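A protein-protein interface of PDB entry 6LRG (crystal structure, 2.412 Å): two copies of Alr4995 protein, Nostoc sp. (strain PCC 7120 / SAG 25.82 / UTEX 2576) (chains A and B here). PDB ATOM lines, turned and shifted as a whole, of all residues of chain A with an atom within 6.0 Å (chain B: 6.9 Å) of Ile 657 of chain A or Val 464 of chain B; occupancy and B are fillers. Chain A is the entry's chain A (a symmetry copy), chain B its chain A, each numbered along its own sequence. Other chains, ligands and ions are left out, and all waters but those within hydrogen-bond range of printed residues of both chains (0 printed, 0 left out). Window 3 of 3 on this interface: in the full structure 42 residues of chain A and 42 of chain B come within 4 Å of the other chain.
Thr 678 of chain A touches none of the printed residues of chain B.
Printed residues of chain B within 4 Å of Asp 679 of chain A: Glu 467.
Val 464 of chain B touches just one residue of chain A: Ile 657.
Of the printed residues of chain A, Glu 467 of chain B touches Asp 679 (3.5 Å).
Of the printed residues of chain A, Ile 657 of chain B touches Val 464 (3.5 Å).
The nearest residue of chain A that does not touch Val 464 of chain B is Asp 679 of chain A (4.8 Å).
The nearest printed residue of chain B that does not touch Asp 679 of chain A is Ser 466 of chain B (4.1 Å).
Hydrophobic or aromatic side chains of chain B within 4 Å of the printed part of chain A: Val 464 and Ile 657.
Among the printed residues, 3 pairs touch across the chains.
Among the printed residues, merely in contact across the chains: Val 464 of chain A with Ile 657 of chain B (3.5 Å), Ile 657 of chain A with Val 464 of chain B (3.5 Å) and Asp 679 of chain A with Glu 467 of chain B (3.5 Å).
Val 464 of chain A touches Ile 657 of chain B, and with the chains exchanged Ile 657 of chain A touches Val 464 of chain B.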
ATOM      1  N   VAL A 464      34.313 -15.165   6.042  1.00  0.00           N
ATOM      2  CA  VAL A 464      33.591 -16.126   6.885  1.00  0.00           C
ATOM      3  C   VAL A 464      34.442 -16.623   8.049  1.00  0.00           C
ATOM      4  O   VAL A 464      35.630 -16.837   7.892  1.00  0.00           O
ATOM      5  CB  VAL A 464      33.118 -17.318   6.045  1.00  0.00           C
ATOM      6  CG1 VAL A 464      32.607 -18.442   6.923  1.00  0.00           C
ATOM      7  CG2 VAL A 464      32.048 -16.861   5.051  1.00  0.00           C
ATOM      8  N   VAL A 655      25.277 -12.352  15.063  1.00  0.00           N
ATOM      9  CA  VAL A 655      25.449 -13.498  14.184  1.00  0.00           C
ATOM     10  C   VAL A 655      24.835 -13.252  12.809  1.00  0.00           C
ATOM     11  O   VAL A 655      23.638 -13.019  12.679  1.00  0.00           O
ATOM     12  CB  VAL A 655      24.834 -14.770  14.793  1.00  0.00           C
ATOM     13  CG1 VAL A 655      25.273 -15.993  14.009  1.00  0.00           C
ATOM     14  CG2 VAL A 655      25.244 -14.905  16.255  1.00  0.00           C
ATOM     15  N   ASP A 656      25.666 -13.316  11.781  1.00  0.00           N
ATOM     16  CA  ASP A 656      25.225 -13.021  10.424  1.00  0.00           C
ATOM     17  C   ASP A 656      26.197 -13.624   9.419  1.00  0.00           C
ATOM     18  O   ASP A 656      27.380 -13.766   9.712  1.00  0.00           O
ATOM     19  CB  ASP A 656      25.121 -11.509  10.224  1.00  0.00           C
ATOM     20  CG  ASP A 656      24.214 -11.127   9.065  1.00  0.00           C
ATOM     21  OD1 ASP A 656      24.642 -11.230   7.888  1.00  0.00           O
ATOM     22  OD2 ASP A 656      23.070 -10.698   9.343  1.00  0.00           O
ATOM     23  N   ILE A 657      25.702 -13.973   8.238  1.00  0.00           N
ATOM     24  CA  ILE A 657      26.550 -14.546   7.194  1.00  0.00           C
ATOM     25  C   ILE A 657      27.298 -13.482   6.366  1.00  0.00           C
ATOM     26  O   ILE A 657      28.306 -13.784   5.725  1.00  0.00           O
ATOM     27  CB  ILE A 657      25.725 -15.439   6.244  1.00  0.00           C
ATOM     28  CG1 ILE A 657      26.648 -16.407   5.506  1.00  0.00           C
ATOM     29  CG2 ILE A 657      24.863 -14.600   5.297  1.00  0.00           C
ATOM     30  CD1 ILE A 657      27.375 -17.385   6.449  1.00  0.00           C
ATOM     31  N   ASN A 658      26.805 -12.243   6.391  1.00  0.00           N
ATOM     32  CA  ASN A 658      27.440 -11.119   5.693  1.00  0.00           C
ATOM     33  C   ASN A 658      28.467 -10.448   6.589  1.00  0.00           C
ATOM     34  O   ASN A 658      28.122  -9.909   7.636  1.00  0.00           O
ATOM     35  CB  ASN A 658      26.386 -10.098   5.239  1.00  0.00           C
ATOM     36  CG  ASN A 658      26.989  -8.884   4.517  1.00  0.00           C
ATOM     37  OD1 ASN A 658      28.062  -8.391   4.869  1.00  0.00           O
ATOM     38  ND2 ASN A 658      26.275  -8.389   3.509  1.00  0.00           N
ATOM     39  N   PRO A 659      29.729 -10.432   6.155  1.00  0.00           N
ATOM     40  CA  PRO A 659      30.789  -9.883   7.003  1.00  0.00           C
ATOM     41  C   PRO A 659      30.587  -8.392   7.260  1.00  0.00           C
ATOM     42  O   PRO A 659      30.974  -7.909   8.327  1.00  0.00           O
ATOM     43  CB  PRO A 659      32.065 -10.129   6.189  1.00  0.00           C
ATOM     44  CG  PRO A 659      31.667 -11.081   5.082  1.00  0.00           C
ATOM     45  CD  PRO A 659      30.224 -10.796   4.819  1.00  0.00           C
ATOM     46  N   VAL A 662      28.169  -7.651  10.326  1.00  0.00           N
ATOM     47  CA  VAL A 662      28.813  -7.986  11.590  1.00  0.00           C
ATOM     48  C   VAL A 662      29.889  -6.971  11.948  1.00  0.00           C
ATOM     49  O   VAL A 662      30.080  -6.637  13.119  1.00  0.00           O
ATOM     50  CB  VAL A 662      29.433  -9.383  11.527  1.00  0.00           C
ATOM     51  CG1 VAL A 662      30.021  -9.773  12.863  1.00  0.00           C
ATOM     52  CG2 VAL A 662      28.390 -10.388  11.093  1.00  0.00           C
ATOM     53  N   VAL A 676      30.362 -13.019  14.810  1.00  0.00           N
ATOM     54  CA  VAL A 676      30.748 -14.250  14.146  1.00  0.00           C
ATOM     55  C   VAL A 676      30.043 -14.310  12.805  1.00  0.00           C
ATOM     56  O   VAL A 676      28.855 -14.034  12.719  1.00  0.00           O
ATOM     57  CB  VAL A 676      30.431 -15.524  15.014  1.00  0.00           C
ATOM     58  CG1 VAL A 676      29.015 -15.508  15.557  1.00  0.00           C
ATOM     59  CG2 VAL A 676      30.670 -16.793  14.222  1.00  0.00           C
ATOM     60  N   VAL A 677      30.794 -14.610  11.750  1.00  0.00           N
ATOM     61  CA  VAL A 677      30.211 -14.753  10.423  1.00  0.00           C
ATOM     62  C   VAL A 677      29.994 -16.219  10.097  1.00  0.00           C
ATOM     63  O   VAL A 677      30.938 -16.939   9.772  1.00  0.00           O
ATOM     64  CB  VAL A 677      31.093 -14.133   9.338  1.00  0.00           C
ATOM     65  CG1 VAL A 677      30.500 -14.416   7.980  1.00  0.00           C
ATOM     66  CG2 VAL A 677      31.243 -12.628   9.557  1.00  0.00           C
ATOM     67  N   THR A 678      28.743 -16.654  10.174  1.00  0.00           N
ATOM     68  CA  THR A 678      28.394 -18.066  10.023  1.00  0.00           C
ATOM     69  C   THR A 678      26.883 -18.145   9.829  1.00  0.00           C
ATOM     70  O   THR A 678      26.181 -17.154  10.024  1.00  0.00           O
ATOM     71  CB  THR A 678      28.842 -18.905  11.266  1.00  0.00           C
ATOM     72  OG1 THR A 678      28.821 -20.306  10.969  1.00  0.00           O
ATOM     73  CG2 THR A 678      27.950 -18.633  12.451  1.00  0.00           C
ATOM     74  N   ASP A 679      26.384 -19.306   9.430  1.00  0.00           N
ATOM     75  CA  ASP A 679      24.945 -19.513   9.336  1.00  0.00           C
ATOM     76  C   ASP A 679      24.331 -19.503  10.741  1.00  0.00           C
ATOM     77  O   ASP A 679      24.774 -20.243  11.625  1.00  0.00           O
ATOM     78  CB  ASP A 679      24.625 -20.831   8.620  1.00  0.00           C
ATOM     79  CG  ASP A 679      23.156 -21.206   8.732  1.00  0.00           C
ATOM     80  OD1 ASP A 679      22.360 -20.699   7.920  1.00  0.00           O
ATOM     81  OD2 ASP A 679      22.787 -21.996   9.632  1.00  0.00           O
ATOM     82  N   VAL A 680      23.303 -18.691  10.949  1.00  0.00           N
ATOM     83  CA  VAL A 680      22.741 -18.539  12.287  1.00  0.00           C
ATOM     84  C   VAL A 680      22.169 -19.849  12.828  1.00  0.00           C
ATOM     85  O   VAL A 680      22.191 -20.086  14.038  1.00  0.00           O
ATOM     86  CB  VAL A 680      21.654 -17.461  12.325  1.00  0.00           C
ATOM     87  CG1 VAL A 680      20.446 -17.879  11.498  1.00  0.00           C
ATOM     88  CG2 VAL A 680      21.260 -17.159  13.763  1.00  0.00           C
ATOM     89  N   VAL B 464      25.237 -19.085   0.673  1.00  0.00           N
ATOM     90  CA  VAL B 464      25.675 -20.034   1.705  1.00  0.00           C
ATOM     91  C   VAL B 464      24.598 -21.061   2.036  1.00  0.00           C
ATOM     92  O   VAL B 464      23.427 -20.729   2.078  1.00  0.00           O
ATOM     93  CB  VAL B 464      26.082 -19.283   2.978  1.00  0.00           C
ATOM     94  CG1 VAL B 464      26.285 -20.236   4.138  1.00  0.00           C
ATOM     95  CG2 VAL B 464      27.344 -18.458   2.712  1.00  0.00           C
ATOM     96  N   SER B 465      24.984 -22.317   2.249  1.00  0.00           N
ATOM     97  CA  SER B 465      24.016 -23.376   2.489  1.00  0.00           C
ATOM     98  C   SER B 465      23.368 -23.290   3.865  1.00  0.00           C
ATOM     99  O   SER B 465      24.032 -23.018   4.861  1.00  0.00           O
ATOM    100  CB  SER B 465      24.670 -24.751   2.329  1.00  0.00           C
ATOM    101  OG  SER B 465      25.300 -24.874   1.074  1.00  0.00           O
ATOM    102  N   SER B 466      22.069 -23.571   3.906  1.00  0.00           N
ATOM    103  CA  SER B 466      21.276 -23.498   5.119  1.00  0.00           C
ATOM    104  C   SER B 466      21.625 -24.579   6.114  1.00  0.00           C
ATOM    105  O   SER B 466      22.267 -25.580   5.768  1.00  0.00           O
ATOM    106  CB  SER B 466      19.806 -23.629   4.780  1.00  0.00           C
ATOM    107  OG  SER B 466      19.549 -24.952   4.371  1.00  0.00           O
ATOM    108  N   GLU B 467      21.154 -24.399   7.343  1.00  0.00           N
ATOM    109  CA  GLU B 467      21.413 -25.381   8.375  1.00  0.00           C
ATOM    110  C   GLU B 467      20.828 -26.715   7.987  1.00  0.00           C
ATOM    111  O   GLU B 467      21.483 -27.745   8.143  1.00  0.00           O
ATOM    112  CB  GLU B 467      20.839 -24.962   9.734  1.00  0.00           C
ATOM    113  CG  GLU B 467      21.102 -26.027  10.801  1.00  0.00           C
ATOM    114  CD  GLU B 467      20.272 -25.862  12.061  1.00  0.00           C
ATOM    115  OE1 GLU B 467      20.305 -26.791  12.904  1.00  0.00           O
ATOM    116  OE2 GLU B 467      19.577 -24.822  12.215  1.00  0.00           O
ATOM    117  N   VAL B 470      22.927 -28.317   5.083  1.00  0.00           N
ATOM    118  CA  VAL B 470      24.179 -28.826   5.612  1.00  0.00           C
ATOM    119  C   VAL B 470      23.937 -30.107   6.403  1.00  0.00           C
ATOM    120  O   VAL B 470      24.640 -31.095   6.209  1.00  0.00           O
ATOM    121  CB  VAL B 470      24.886 -27.799   6.513  1.00  0.00           C
ATOM    122  CG1 VAL B 470      26.110 -28.414   7.116  1.00  0.00           C
ATOM    123  CG2 VAL B 470      25.270 -26.573   5.704  1.00  0.00           C
ATOM    124  N   ILE B 657      33.511 -22.538   0.696  1.00  0.00           N
ATOM    125  CA  ILE B 657      32.750 -21.383   1.169  1.00  0.00           C
ATOM    126  C   ILE B 657      32.300 -20.444   0.031  1.00  0.00           C
ATOM    127  O   ILE B 657      31.364 -19.662   0.201  1.00  0.00           O
ATOM    128  CB  ILE B 657      33.563 -20.574   2.200  1.00  0.00           C
ATOM    129  CG1 ILE B 657      32.623 -19.713   3.044  1.00  0.00           C
ATOM    130  CG2 ILE B 657      34.671 -19.761   1.526  1.00  0.00           C
ATOM    131  CD1 ILE B 657      31.628 -20.543   3.876  1.00  0.00           C
ATOM    132  N   PRO B 659      30.411 -19.851  -3.335  1.00  0.00           N
ATOM    133  CA  PRO B 659      29.332 -20.526  -4.059  1.00  0.00           C
ATOM    134  C   PRO B 659      29.715 -20.800  -5.512  1.00  0.00           C
ATOM    135  O   PRO B 659      29.253 -21.793  -6.077  1.00  0.00           O
ATOM    136  CB  PRO B 659      28.168 -19.531  -3.980  1.00  0.00           C
ATOM    137  CG  PRO B 659      28.577 -18.504  -2.947  1.00  0.00           C
ATOM    138  CD  PRO B 659      30.069 -18.458  -3.009  1.00  0.00           C
ATOM    139  N   VAL B 676      28.132 -28.331  -1.126  1.00  0.00           N
ATOM    140  CA  VAL B 676      27.668 -27.625   0.054  1.00  0.00           C
ATOM    141  C   VAL B 676      28.545 -26.406   0.256  1.00  0.00           C
ATOM    142  O   VAL B 676      29.761 -26.496   0.161  1.00  0.00           O
ATOM    143  CB  VAL B 676      27.659 -28.540   1.334  1.00  0.00           C
ATOM    144  CG1 VAL B 676      28.966 -29.289   1.511  1.00  0.00           C
ATOM    145  CG2 VAL B 676      27.352 -27.731   2.578  1.00  0.00           C
ATOM    146  N   VAL B 677      27.921 -25.253   0.474  1.00  0.00           N
ATOM    147  CA  VAL B 677      28.665 -24.029   0.739  1.00  0.00           C
ATOM    148  C   VAL B 677      28.705 -23.749   2.231  1.00  0.00           C
ATOM    149  O   VAL B 677      27.723 -23.291   2.814  1.00  0.00           O
ATOM    150  CB  VAL B 677      28.056 -22.819   0.029  1.00  0.00           C
ATOM    151  CG1 VAL B 677      28.792 -21.568   0.436  1.00  0.00           C
ATOM    152  CG2 VAL B 677      28.102 -23.003  -1.487  1.00  0.00           C
ATOM    153  N   THR B 678      29.852 -24.015   2.842  1.00  0.00           N
ATOM    154  CA  THR B 678      30.004 -23.929   4.294  1.00  0.00           C
ATOM    155  C   THR B 678      31.498 -23.964   4.601  1.00  0.00           C
ATOM    156  O   THR B 678      32.304 -24.255   3.718  1.00  0.00           O
ATOM    157  CB  THR B 678      29.258 -25.097   5.021  1.00  0.00           C
ATOM    158  OG1 THR B 678      29.112 -24.817   6.419  1.00  0.00           O
ATOM    159  CG2 THR B 678      29.996 -26.400   4.849  1.00  0.00           C
ATOM    160  N   ASP B 679      31.871 -23.652   5.833  1.00  0.00           N
ATOM    161  CA  ASP B 679      33.260 -23.776   6.252  1.00  0.00           C
ATOM    162  C   ASP B 679      33.656 -25.258   6.292  1.00  0.00           C
ATOM    163  O   ASP B 679      32.982 -26.071   6.932  1.00  0.00           O
ATOM    164  CB  ASP B 679      33.481 -23.127   7.624  1.00  0.00           C
ATOM    165  CG  ASP B 679      34.844 -23.460   8.207  1.00  0.00           C
ATOM    166  OD1 ASP B 679      35.819 -22.773   7.847  1.00  0.00           O
ATOM    167  OD2 ASP B 679      34.955 -24.411   9.016  1.00  0.00           O
